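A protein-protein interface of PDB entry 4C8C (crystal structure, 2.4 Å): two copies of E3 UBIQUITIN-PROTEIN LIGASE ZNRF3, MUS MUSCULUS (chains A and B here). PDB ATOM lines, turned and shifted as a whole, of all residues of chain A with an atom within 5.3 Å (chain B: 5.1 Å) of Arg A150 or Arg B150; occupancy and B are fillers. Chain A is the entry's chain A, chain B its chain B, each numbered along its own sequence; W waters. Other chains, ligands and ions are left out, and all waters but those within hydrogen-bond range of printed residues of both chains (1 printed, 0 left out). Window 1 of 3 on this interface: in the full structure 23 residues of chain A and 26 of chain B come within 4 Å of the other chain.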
ATOM      1  N   GLU A  10     -12.795  15.150  -8.102  1.00  0.00           N
ATOM      2  CA  GLU A  10     -13.533  16.379  -7.743  1.00  0.00           C
ATOM      3  C   GLU A  10     -15.053  16.319  -8.032  1.00  0.00           C
ATOM      4  O   GLU A  10     -15.511  16.009  -9.156  1.00  0.00           O
ATOM      5  CB  GLU A  10     -12.968  17.569  -8.517  1.00  0.00           C
ATOM      6  CG  GLU A  10     -11.894  18.323  -7.757  1.00  0.00           C
ATOM      7  CD  GLU A  10     -11.278  19.510  -8.510  1.00  0.00           C
ATOM      8  OE1 GLU A  10     -11.433  19.650  -9.765  1.00  0.00           O
ATOM      9  OE2 GLU A  10     -10.595  20.303  -7.806  1.00  0.00           O
ATOM     10  N   VAL A  11     -15.840  16.640  -7.027  1.00  0.00           N
ATOM     11  CA  VAL A  11     -17.266  16.656  -7.203  1.00  0.00           C
ATOM     12  C   VAL A  11     -17.659  18.097  -7.123  1.00  0.00           C
ATOM     13  O   VAL A  11     -17.396  18.719  -6.097  1.00  0.00           O
ATOM     14  CB  VAL A  11     -17.993  15.941  -6.096  1.00  0.00           C
ATOM     15  CG1 VAL A  11     -19.484  16.042  -6.338  1.00  0.00           C
ATOM     16  CG2 VAL A  11     -17.627  14.500  -6.077  1.00  0.00           C
ATOM     17  N   VAL A  12     -18.293  18.581  -8.197  1.00  0.00           N
ATOM     18  CA  VAL A  12     -18.608  19.986  -8.440  1.00  0.00           C
ATOM     19  C   VAL A  12     -20.129  20.184  -8.348  1.00  0.00           C
ATOM     20  O   VAL A  12     -20.898  19.514  -9.031  1.00  0.00           O
ATOM     21  CB  VAL A  12     -18.165  20.390  -9.847  1.00  0.00           C
ATOM     22  CG1 VAL A  12     -18.186  21.888 -10.025  1.00  0.00           C
ATOM     23  CG2 VAL A  12     -16.758  19.877 -10.139  1.00  0.00           C
ATOM     24  N   PHE A  14     -23.180  23.180  -8.775  1.00  0.00           N
ATOM     25  CA  PHE A  14     -23.240  24.403  -9.545  1.00  0.00           C
ATOM     26  C   PHE A  14     -24.641  25.009  -9.529  1.00  0.00           C
ATOM     27  O   PHE A  14     -25.638  24.281  -9.666  1.00  0.00           O
ATOM     28  CB  PHE A  14     -22.768  24.149 -10.987  1.00  0.00           C
ATOM     29  CG  PHE A  14     -23.332  22.897 -11.606  1.00  0.00           C
ATOM     30  CD1 PHE A  14     -24.563  22.908 -12.243  1.00  0.00           C
ATOM     31  CD2 PHE A  14     -22.620  21.688 -11.561  1.00  0.00           C
ATOM     32  CE1 PHE A  14     -25.085  21.751 -12.814  1.00  0.00           C
ATOM     33  CE2 PHE A  14     -23.143  20.533 -12.132  1.00  0.00           C
ATOM     34  CZ  PHE A  14     -24.382  20.568 -12.748  1.00  0.00           C
ATOM     35  N   GLU A  43     -14.189  13.184 -16.958  1.00  0.00           N
ATOM     36  CA  GLU A  43     -15.060  14.085 -16.231  1.00  0.00           C
ATOM     37  C   GLU A  43     -16.440  13.971 -16.915  1.00  0.00           C
ATOM     38  O   GLU A  43     -16.476  13.624 -18.070  1.00  0.00           O
ATOM     39  CB  GLU A  43     -14.535  15.500 -16.382  1.00  0.00           C
ATOM     40  CG  GLU A  43     -15.613  16.569 -16.581  1.00  0.00           C
ATOM     41  CD  GLU A  43     -14.991  17.928 -16.769  1.00  0.00           C
ATOM     42  OE1 GLU A  43     -13.793  17.982 -17.107  1.00  0.00           O
ATOM     43  OE2 GLU A  43     -15.677  18.946 -16.597  1.00  0.00           O
ATOM     44  N   GLY A  44     -17.528  14.278 -16.221  1.00  0.00           N
ATOM     45  CA  GLY A  44     -18.877  13.986 -16.760  1.00  0.00           C
ATOM     46  C   GLY A  44     -19.809  14.029 -15.592  1.00  0.00           C
ATOM     47  O   GLY A  44     -19.376  13.948 -14.460  1.00  0.00           O
ATOM     48  N   GLU A  45     -21.075  14.232 -15.860  1.00  0.00           N
ATOM     49  CA  GLU A  45     -22.133  14.213 -14.837  1.00  0.00           C
ATOM     50  C   GLU A  45     -22.366  12.874 -14.123  1.00  0.00           C
ATOM     51  O   GLU A  45     -22.310  11.804 -14.731  1.00  0.00           O
ATOM     52  CB  GLU A  45     -23.483  14.616 -15.472  1.00  0.00           C
ATOM     53  CG  GLU A  45     -24.649  14.675 -14.474  1.00  0.00           C
ATOM     54  CD  GLU A  45     -25.727  15.714 -14.847  1.00  0.00           C
ATOM     55  OE1 GLU A  45     -26.327  15.595 -15.947  1.00  0.00           O
ATOM     56  OE2 GLU A  45     -25.961  16.657 -14.044  1.00  0.00           O
ATOM     57  N   ILE A  46     -22.757  12.966 -12.862  1.00  0.00           N
ATOM     58  CA  ILE A  46     -22.925  11.821 -12.008  1.00  0.00           C
ATOM     59  C   ILE A  46     -24.285  11.148 -12.070  1.00  0.00           C
ATOM     60  O   ILE A  46     -25.346  11.777 -11.981  1.00  0.00           O
ATOM     61  CB  ILE A  46     -22.601  12.194 -10.540  1.00  0.00           C
ATOM     62  CG1 ILE A  46     -21.107  12.411 -10.390  1.00  0.00           C
ATOM     63  CG2 ILE A  46     -23.046  11.091  -9.571  1.00  0.00           C
ATOM     64  CD1 ILE A  46     -20.766  13.023  -9.042  1.00  0.00           C
ATOM     65  N   TYR A  66     -24.820  10.159 -23.176  1.00  0.00           N
ATOM     66  CA  TYR A  66     -23.471   9.629 -23.313  1.00  0.00           C
ATOM     67  C   TYR A  66     -22.463  10.482 -22.541  1.00  0.00           C
ATOM     68  O   TYR A  66     -22.239  11.679 -22.798  1.00  0.00           O
ATOM     69  CB  TYR A  66     -23.026   9.517 -24.747  1.00  0.00           C
ATOM     70  CG  TYR A  66     -21.658   8.910 -24.823  1.00  0.00           C
ATOM     71  CD1 TYR A  66     -21.493   7.519 -24.814  1.00  0.00           C
ATOM     72  CD2 TYR A  66     -20.524   9.697 -24.866  1.00  0.00           C
ATOM     73  CE1 TYR A  66     -20.235   6.932 -24.851  1.00  0.00           C
ATOM     74  CE2 TYR A  66     -19.241   9.113 -24.901  1.00  0.00           C
ATOM     75  CZ  TYR A  66     -19.103   7.736 -24.884  1.00  0.00           C
ATOM     76  OH  TYR A  66     -17.856   7.151 -24.938  1.00  0.00           O
ATOM     77  N   GLY A  67     -21.829   9.832 -21.600  1.00  0.00           N
ATOM     78  CA  GLY A  67     -20.662  10.393 -20.988  1.00  0.00           C
ATOM     79  C   GLY A  67     -20.975  10.748 -19.571  1.00  0.00           C
ATOM     80  O   GLY A  67     -20.562  11.757 -19.135  1.00  0.00           O
ATOM     81  N   THR A 100     -18.697   7.461 -18.985  1.00  0.00           N
ATOM     82  CA  THR A 100     -17.336   7.884 -19.388  1.00  0.00           C
ATOM     83  C   THR A 100     -16.331   7.286 -18.383  1.00  0.00           C
ATOM     84  O   THR A 100     -15.197   7.043 -18.744  1.00  0.00           O
ATOM     85  CB  THR A 100     -17.116   9.419 -19.400  1.00  0.00           C
ATOM     86  OG1 THR A 100     -15.813   9.712 -19.915  1.00  0.00           O
ATOM     87  CG2 THR A 100     -17.205  10.085 -17.972  1.00  0.00           C
ATOM     88  N   VAL A 148     -27.568  17.478  -8.143  1.00  0.00           N
ATOM     89  CA  VAL A 148     -27.041  17.149  -9.463  1.00  0.00           C
ATOM     90  C   VAL A 148     -25.566  17.656  -9.576  1.00  0.00           C
ATOM     91  O   VAL A 148     -25.236  18.783  -9.177  1.00  0.00           O
ATOM     92  CB  VAL A 148     -28.037  17.700 -10.542  1.00  0.00           C
ATOM     93  CG1 VAL A 148     -27.575  19.017 -11.175  1.00  0.00           C
ATOM     94  CG2 VAL A 148     -28.332  16.640 -11.605  1.00  0.00           C
ATOM     95  N   ALA A 149     -24.670  16.821 -10.084  1.00  0.00           N
ATOM     96  CA  ALA A 149     -23.230  17.068  -9.880  1.00  0.00           C
ATOM     97  C   ALA A 149     -22.399  16.625 -11.042  1.00  0.00           C
ATOM     98  O   ALA A 149     -22.818  15.810 -11.859  1.00  0.00           O
ATOM     99  CB  ALA A 149     -22.780  16.365  -8.616  1.00  0.00           C
ATOM    100  N   ARG A 150     -21.242  17.239 -11.155  1.00  0.00           N
ATOM    101  CA  ARG A 150     -20.244  16.812 -12.106  1.00  0.00           C
ATOM    102  C   ARG A 150     -19.069  16.217 -11.321  1.00  0.00           C
ATOM    103  O   ARG A 150     -18.763  16.624 -10.217  1.00  0.00           O
ATOM    104  CB  ARG A 150     -19.775  17.984 -12.969  1.00  0.00           C
ATOM    105  CG  ARG A 150     -18.895  17.559 -14.147  1.00  0.00           C
ATOM    106  CD  ARG A 150     -18.637  18.694 -15.127  1.00  0.00           C
ATOM    107  NE  ARG A 150     -18.332  18.247 -16.518  1.00  0.00           N
ATOM    108  CZ  ARG A 150     -19.231  17.785 -17.389  1.00  0.00           C
ATOM    109  NH1 ARG A 150     -20.501  17.647 -17.031  1.00  0.00           N
ATOM    110  NH2 ARG A 150     -18.867  17.407 -18.615  1.00  0.00           N
ATOM    111  N   ALA A 151     -18.429  15.240 -11.910  1.00  0.00           N
ATOM    112  CA  ALA A 151     -17.258  14.643 -11.346  1.00  0.00           C
ATOM    113  C   ALA A 151     -16.081  14.803 -12.324  1.00  0.00           C
ATOM    114  O   ALA A 151     -16.259  14.669 -13.536  1.00  0.00           O
ATOM    115  CB  ALA A 151     -17.522  13.179 -11.067  1.00  0.00           C
ATOM    116  N   ARG A 152     -14.905  15.136 -11.787  1.00  0.00           N
ATOM    117  CA  ARG A 152     -13.658  15.083 -12.560  1.00  0.00           C
ATOM    118  C   ARG A 152     -12.604  14.189 -11.905  1.00  0.00           C
ATOM    119  O   ARG A 152     -12.258  14.362 -10.721  1.00  0.00           O
ATOM    120  CB  ARG A 152     -13.072  16.454 -12.705  1.00  0.00           C
ATOM    121  CG  ARG A 152     -14.094  17.578 -12.761  1.00  0.00           C
ATOM    122  CD  ARG A 152     -13.379  18.818 -13.274  1.00  0.00           C
ATOM    123  NE  ARG A 152     -14.226  19.984 -13.489  1.00  0.00           N
ATOM    124  CZ  ARG A 152     -14.293  21.038 -12.665  1.00  0.00           C
ATOM    125  NH1 ARG A 152     -13.582  21.107 -11.492  1.00  0.00           N
ATOM    126  NH2 ARG A 152     -15.093  22.044 -13.009  1.00  0.00           N
ATOM    127  N   GLU B  10      -9.663  14.184 -28.145  1.00  0.00           N
ATOM    128  CA  GLU B  10     -10.523  13.221 -28.824  1.00  0.00           C
ATOM    129  C   GLU B  10     -11.938  13.822 -28.994  1.00  0.00           C
ATOM    130  O   GLU B  10     -12.540  14.331 -28.031  1.00  0.00           O
ATOM    131  CB  GLU B  10     -10.611  11.909 -28.037  1.00  0.00           C
ATOM    132  CG  GLU B  10      -9.295  11.150 -27.839  1.00  0.00           C
ATOM    133  CD  GLU B  10      -9.486   9.679 -27.406  1.00  0.00           C
ATOM    134  OE1 GLU B  10     -10.185   9.410 -26.397  1.00  0.00           O
ATOM    135  OE2 GLU B  10      -8.913   8.786 -28.076  1.00  0.00           O
ATOM    136  N   VAL B  11     -12.469  13.756 -30.210  1.00  0.00           N
ATOM    137  CA  VAL B  11     -13.865  14.094 -30.434  1.00  0.00           C
ATOM    138  C   VAL B  11     -14.631  12.825 -30.595  1.00  0.00           C
ATOM    139  O   VAL B  11     -14.269  12.025 -31.441  1.00  0.00           O
ATOM    140  CB  VAL B  11     -14.140  14.901 -31.708  1.00  0.00           C
ATOM    141  CG1 VAL B  11     -15.573  15.412 -31.691  1.00  0.00           C
ATOM    142  CG2 VAL B  11     -13.234  16.097 -31.793  1.00  0.00           C
ATOM    143  N   VAL B  12     -15.727  12.694 -29.841  1.00  0.00           N
ATOM    144  CA  VAL B  12     -16.516  11.479 -29.825  1.00  0.00           C
ATOM    145  C   VAL B  12     -17.909  11.637 -30.432  1.00  0.00           C
ATOM    146  O   VAL B  12     -18.730  12.457 -29.990  1.00  0.00           O
ATOM    147  CB  VAL B  12     -16.670  10.946 -28.395  1.00  0.00           C
ATOM    148  CG1 VAL B  12     -17.464   9.637 -28.404  1.00  0.00           C
ATOM    149  CG2 VAL B  12     -15.300  10.747 -27.756  1.00  0.00           C
ATOM    150  N   PHE B  14     -21.426   9.418 -31.124  1.00  0.00           N
ATOM    151  CA  PHE B  14     -22.051   8.288 -30.509  1.00  0.00           C
ATOM    152  C   PHE B  14     -23.530   8.106 -30.850  1.00  0.00           C
ATOM    153  O   PHE B  14     -24.288   9.059 -31.090  1.00  0.00           O
ATOM    154  CB  PHE B  14     -21.880   8.438 -29.026  1.00  0.00           C
ATOM    155  CG  PHE B  14     -22.374   9.744 -28.505  1.00  0.00           C
ATOM    156  CD1 PHE B  14     -23.729   9.934 -28.243  1.00  0.00           C
ATOM    157  CD2 PHE B  14     -21.491  10.785 -28.257  1.00  0.00           C
ATOM    158  CE1 PHE B  14     -24.190  11.144 -27.748  1.00  0.00           C
ATOM    159  CE2 PHE B  14     -21.952  11.999 -27.767  1.00  0.00           C
ATOM    160  CZ  PHE B  14     -23.301  12.180 -27.521  1.00  0.00           C
ATOM    161  N   GLU B  43     -13.293  17.106 -20.142  1.00  0.00           N
ATOM    162  CA  GLU B  43     -14.223  16.381 -21.008  1.00  0.00           C
ATOM    163  C   GLU B  43     -15.617  17.030 -20.854  1.00  0.00           C
ATOM    164  O   GLU B  43     -16.000  17.492 -19.757  1.00  0.00           O
ATOM    165  CB  GLU B  43     -14.362  14.898 -20.559  1.00  0.00           C
ATOM    166  CG  GLU B  43     -15.368  14.129 -21.385  1.00  0.00           C
ATOM    167  CD  GLU B  43     -15.557  12.694 -20.994  1.00  0.00           C
ATOM    168  OE1 GLU B  43     -15.057  12.255 -19.965  1.00  0.00           O
ATOM    169  OE2 GLU B  43     -16.266  11.984 -21.754  1.00  0.00           O
ATOM    170  N   GLY B  44     -16.389  17.009 -21.925  1.00  0.00           N
ATOM    171  CA  GLY B  44     -17.628  17.747 -21.949  1.00  0.00           C
ATOM    172  C   GLY B  44     -18.162  17.745 -23.333  1.00  0.00           C
ATOM    173  O   GLY B  44     -17.409  17.533 -24.294  1.00  0.00           O
ATOM    174  N   GLU B  45     -19.475  17.904 -23.412  1.00  0.00           N
ATOM    175  CA  GLU B  45     -20.176  18.076 -24.669  1.00  0.00           C
ATOM    176  C   GLU B  45     -19.619  19.329 -25.331  1.00  0.00           C
ATOM    177  O   GLU B  45     -19.201  20.293 -24.639  1.00  0.00           O
ATOM    178  CB  GLU B  45     -21.711  18.239 -24.434  1.00  0.00           C
ATOM    179  CG  GLU B  45     -22.555  18.032 -25.729  1.00  0.00           C
ATOM    180  CD  GLU B  45     -24.107  18.009 -25.579  1.00  0.00           C
ATOM    181  OE1 GLU B  45     -24.664  18.146 -24.456  1.00  0.00           O
ATOM    182  OE2 GLU B  45     -24.790  17.845 -26.631  1.00  0.00           O
ATOM    183  N   ILE B  46     -19.607  19.316 -26.657  1.00  0.00           N
ATOM    184  CA  ILE B  46     -19.193  20.457 -27.470  1.00  0.00           C
ATOM    185  C   ILE B  46     -20.343  21.424 -27.731  1.00  0.00           C
ATOM    186  O   ILE B  46     -21.398  21.036 -28.203  1.00  0.00           O
ATOM    187  CB  ILE B  46     -18.626  19.987 -28.819  1.00  0.00           C
ATOM    188  CG1 ILE B  46     -17.200  19.437 -28.627  1.00  0.00           C
ATOM    189  CG2 ILE B  46     -18.650  21.105 -29.889  1.00  0.00           C
ATOM    190  CD1 ILE B  46     -16.798  18.544 -29.779  1.00  0.00           C
ATOM    191  N   TYR B  66     -24.039  23.123 -17.396  1.00  0.00           N
ATOM    192  CA  TYR B  66     -22.706  23.256 -16.817  1.00  0.00           C
ATOM    193  C   TYR B  66     -21.774  22.120 -17.283  1.00  0.00           C
ATOM    194  O   TYR B  66     -22.126  20.960 -17.200  1.00  0.00           O
ATOM    195  CB  TYR B  66     -22.728  23.313 -15.300  1.00  0.00           C
ATOM    196  CG  TYR B  66     -21.318  23.436 -14.757  1.00  0.00           C
ATOM    197  CD1 TYR B  66     -20.730  24.675 -14.610  1.00  0.00           C
ATOM    198  CD2 TYR B  66     -20.553  22.312 -14.447  1.00  0.00           C
ATOM    199  CE1 TYR B  66     -19.438  24.814 -14.128  1.00  0.00           C
ATOM    200  CE2 TYR B  66     -19.262  22.439 -13.978  1.00  0.00           C
ATOM    201  CZ  TYR B  66     -18.700  23.690 -13.824  1.00  0.00           C
ATOM    202  OH  TYR B  66     -17.399  23.859 -13.360  1.00  0.00           O
ATOM    203  N   GLY B  67     -20.588  22.468 -17.785  1.00  0.00           N
ATOM    204  CA  GLY B  67     -19.594  21.455 -18.105  1.00  0.00           C
ATOM    205  C   GLY B  67     -19.367  21.261 -19.578  1.00  0.00           C
ATOM    206  O   GLY B  67     -18.723  20.307 -20.025  1.00  0.00           O
ATOM    207  N   THR B 100     -16.550  23.858 -19.281  1.00  0.00           N
ATOM    208  CA  THR B 100     -15.514  23.136 -18.586  1.00  0.00           C
ATOM    209  C   THR B 100     -14.095  23.349 -19.180  1.00  0.00           C
ATOM    210  O   THR B 100     -13.161  23.169 -18.486  1.00  0.00           O
ATOM    211  CB  THR B 100     -15.711  21.614 -18.501  1.00  0.00           C
ATOM    212  OG1 THR B 100     -14.667  21.127 -17.607  1.00  0.00           O
ATOM    213  CG2 THR B 100     -15.548  20.978 -19.867  1.00  0.00           C
ATOM    214  N   VAL B 148     -24.386  16.099 -32.139  1.00  0.00           N
ATOM    215  CA  VAL B 148     -23.870  16.280 -30.794  1.00  0.00           C
ATOM    216  C   VAL B 148     -22.556  15.489 -30.665  1.00  0.00           C
ATOM    217  O   VAL B 148     -22.405  14.359 -31.178  1.00  0.00           O
ATOM    218  CB  VAL B 148     -24.906  15.891 -29.721  1.00  0.00           C
ATOM    219  CG1 VAL B 148     -26.093  16.854 -29.783  1.00  0.00           C
ATOM    220  CG2 VAL B 148     -25.378  14.447 -29.872  1.00  0.00           C
ATOM    221  N   ALA B 149     -21.579  16.103 -30.024  1.00  0.00           N
ATOM    222  CA  ALA B 149     -20.290  15.475 -29.888  1.00  0.00           C
ATOM    223  C   ALA B 149     -19.754  15.705 -28.511  1.00  0.00           C
ATOM    224  O   ALA B 149     -20.012  16.729 -27.907  1.00  0.00           O
ATOM    225  CB  ALA B 149     -19.356  16.067 -30.899  1.00  0.00           C
ATOM    226  N   ARG B 150     -18.966  14.759 -28.031  1.00  0.00           N
ATOM    227  CA  ARG B 150     -18.247  14.946 -26.801  1.00  0.00           C
ATOM    228  C   ARG B 150     -16.749  15.217 -27.089  1.00  0.00           C
ATOM    229  O   ARG B 150     -16.161  14.702 -28.043  1.00  0.00           O
ATOM    230  CB  ARG B 150     -18.468  13.734 -25.906  1.00  0.00           C
ATOM    231  CG  ARG B 150     -18.216  14.041 -24.439  1.00  0.00           C
ATOM    232  CD  ARG B 150     -18.960  13.102 -23.524  1.00  0.00           C
ATOM    233  NE  ARG B 150     -18.480  13.238 -22.188  1.00  0.00           N
ATOM    234  CZ  ARG B 150     -19.019  13.963 -21.224  1.00  0.00           C
ATOM    235  NH1 ARG B 150     -20.153  14.675 -21.410  1.00  0.00           N
ATOM    236  NH2 ARG B 150     -18.409  13.954 -20.022  1.00  0.00           N
ATOM    237  N   ALA B 151     -16.147  16.051 -26.266  1.00  0.00           N
ATOM    238  CA  ALA B 151     -14.720  16.350 -26.399  1.00  0.00           C
ATOM    239  C   ALA B 151     -13.979  15.864 -25.182  1.00  0.00           C
ATOM    240  O   ALA B 151     -14.377  16.211 -24.054  1.00  0.00           O
ATOM    241  CB  ALA B 151     -14.499  17.839 -26.571  1.00  0.00           C
ATOM    242  N   ARG B 152     -12.966  15.019 -25.384  1.00  0.00           N
ATOM    243  CA  ARG B 152     -12.049  14.699 -24.250  1.00  0.00           C
ATOM    244  C   ARG B 152     -10.671  15.312 -24.460  1.00  0.00           C
ATOM    245  O   ARG B 152     -10.000  15.032 -25.454  1.00  0.00           O
ATOM    246  CB  ARG B 152     -11.895  13.224 -24.060  1.00  0.00           C
ATOM    247  CG  ARG B 152     -13.204  12.498 -24.092  1.00  0.00           C
ATOM    248  CD  ARG B 152     -13.040  11.171 -23.434  1.00  0.00           C
ATOM    249  NE  ARG B 152     -14.087  10.217 -23.736  1.00  0.00           N
ATOM    250  CZ  ARG B 152     -14.043   9.295 -24.688  1.00  0.00           C
ATOM    251  NH1 ARG B 152     -12.998   9.168 -25.550  1.00  0.00           N
ATOM    252  NH2 ARG B 152     -15.066   8.460 -24.772  1.00  0.00           N
HETATM  253  O   HOH W   1     -21.742  13.788 -24.282  1.00  0.00           O
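O of Gly B67 is in hydrogen-bond range of NH2 of Arg A150 (3.2 Å).
N of Glu B43 is in hydrogen-bond range of OE1 of Glu A43 (3.2 Å).
OG1 of Thr B100 lies within hydrogen-bond range of OE2 of Glu A43 (2.6 Å).
The backbone carbonyl oxygen of Gly A67 is in hydrogen-bond range of the guanidinium group of Arg B150 (3.2 Å).
OH of Tyr A66 sits at hydrogen-bond distance from NH2 of Arg B152 (3.1 Å).
The guanidinium group (NH2) of Arg B150 lies within hydrogen-bond range of the backbone carbonyl oxygen (O) of Glu A43 (2.8 Å).
OG1 of Thr A100 lies within hydrogen-bond range of OE1 of Glu B43, at 2.7 Å.
OH of Tyr B66 lies within hydrogen-bond range of NH2 of Arg A152 (3.0 Å).
The backbone carbonyl oxygen (O) of Glu B43 lies within hydrogen-bond range of the guanidinium group (NH2) of Arg A150 (3.1 Å).
The backbone carbonyl oxygen of Arg A150 lies within hydrogen-bond range of the backbone NH of Val A12 (2.9 Å).
The side-chain carboxylate (OE2) of Glu A43 lies within salt-bridge range of the guanidinium group (NE) of Arg A152, 3.6 Å away.
The backbone carbonyl oxygen (O) of Gly B44 is in hydrogen-bond range of the backbone NH (N) of Ala B151, at 2.8 Å.
The side-chain carboxylate (OE2) of Glu B43 lies within salt-bridge range of the guanidinium group (NE) of Arg B150 (2.6 Å).
The side-chain carboxylate (OE2) of Glu A43 is in salt-bridge range of the guanidinium group (NE) of Arg A150 (2.7 Å).
The side-chain carboxylate of Glu B10 is in salt-bridge range of the guanidinium group of Arg B152 (2.9 Å).
Among the printed residues, pairs that only touch across the chains: Gly A44 with Arg B150 (3.3 Å), Arg A150 with Gly B44 (3.6 Å), Phe A14 with Tyr B66 (3.6 Å), Tyr A66 with Phe B14 (3.6 Å), Tyr A66 with Arg B150 (3.6 Å), Arg A150 with Tyr B66 (3.7 Å), Arg A150 with Arg B150 (3.8 Å), Val A12 with Tyr B66 (3.95 Å) and Tyr A66 with Val B12 (3.96 Å).
Arg A150 touches just these residues of chain B: Glu B43, Gly B44, Tyr B66, Gly B67 and Arg B150.
Arg B150 touches just these residues of chain A: Glu A43 (2.8 Å), Gly A44 (3.3 Å), Tyr A66 (3.6 Å), Gly A67 (3.2 Å) and Arg A150 (3.8 Å).
Printed residues of chain B within 4 Å of Arg A152: Tyr B66 (3.0 Å).
Printed residues of chain A within 4 Å of Tyr B66: Val A12 (3.95 Å), Phe A14 (3.6 Å), Arg A150 (3.7 Å) and Arg A152 (3.0 Å).
Printed residues of chain A within 4 Å of Thr B100: Glu A43 (2.6 Å).
Of the printed residues of chain A, Phe B14 touches Tyr A66 (3.6 Å).
Val A148 touches none of the printed residues of chain B.
The nearest residue of chain B that does not touch Arg A150 is Thr B100 (4.7 Å).
The nearest residue of chain A that does not touch Arg B150 is Thr A100 (4.5 Å).
Of the 16 printed residues of chain A, 9 touch a printed residue of chain B.
Hydrophobic or aromatic side chains of chain A that line the printed part of chain B: Val A12, Phe A14 and Tyr A66.
Hydrophobic or aromatic side chains of chain B that line the printed part of chain A: Val B12, Phe B14 and Tyr B66.
Along chain B the printed residues that touch a printed residue of chain A span positions 12 to 152.
Among the printed residues, no Asp or Glu carboxylate lies within 4 Å of a Lys or Arg side-chain nitrogen of the other chain.
Phe A14 touches Tyr B66, and with the chains exchanged Tyr A66 touches Phe B14.
Glu A43 touches its own counterpart, Glu B43.
Tyr A66 touches Arg B152, and with the chains exchanged Arg A152 touches Tyr B66.
Arg B150 touches its own counterpart, Arg A150.
16 positions are printed for both chains.
Water W1 lies within hydrogen-bond range of O of Tyr A66 (2.6 Å) and NH1 of Arg B150 (3.4 Å).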
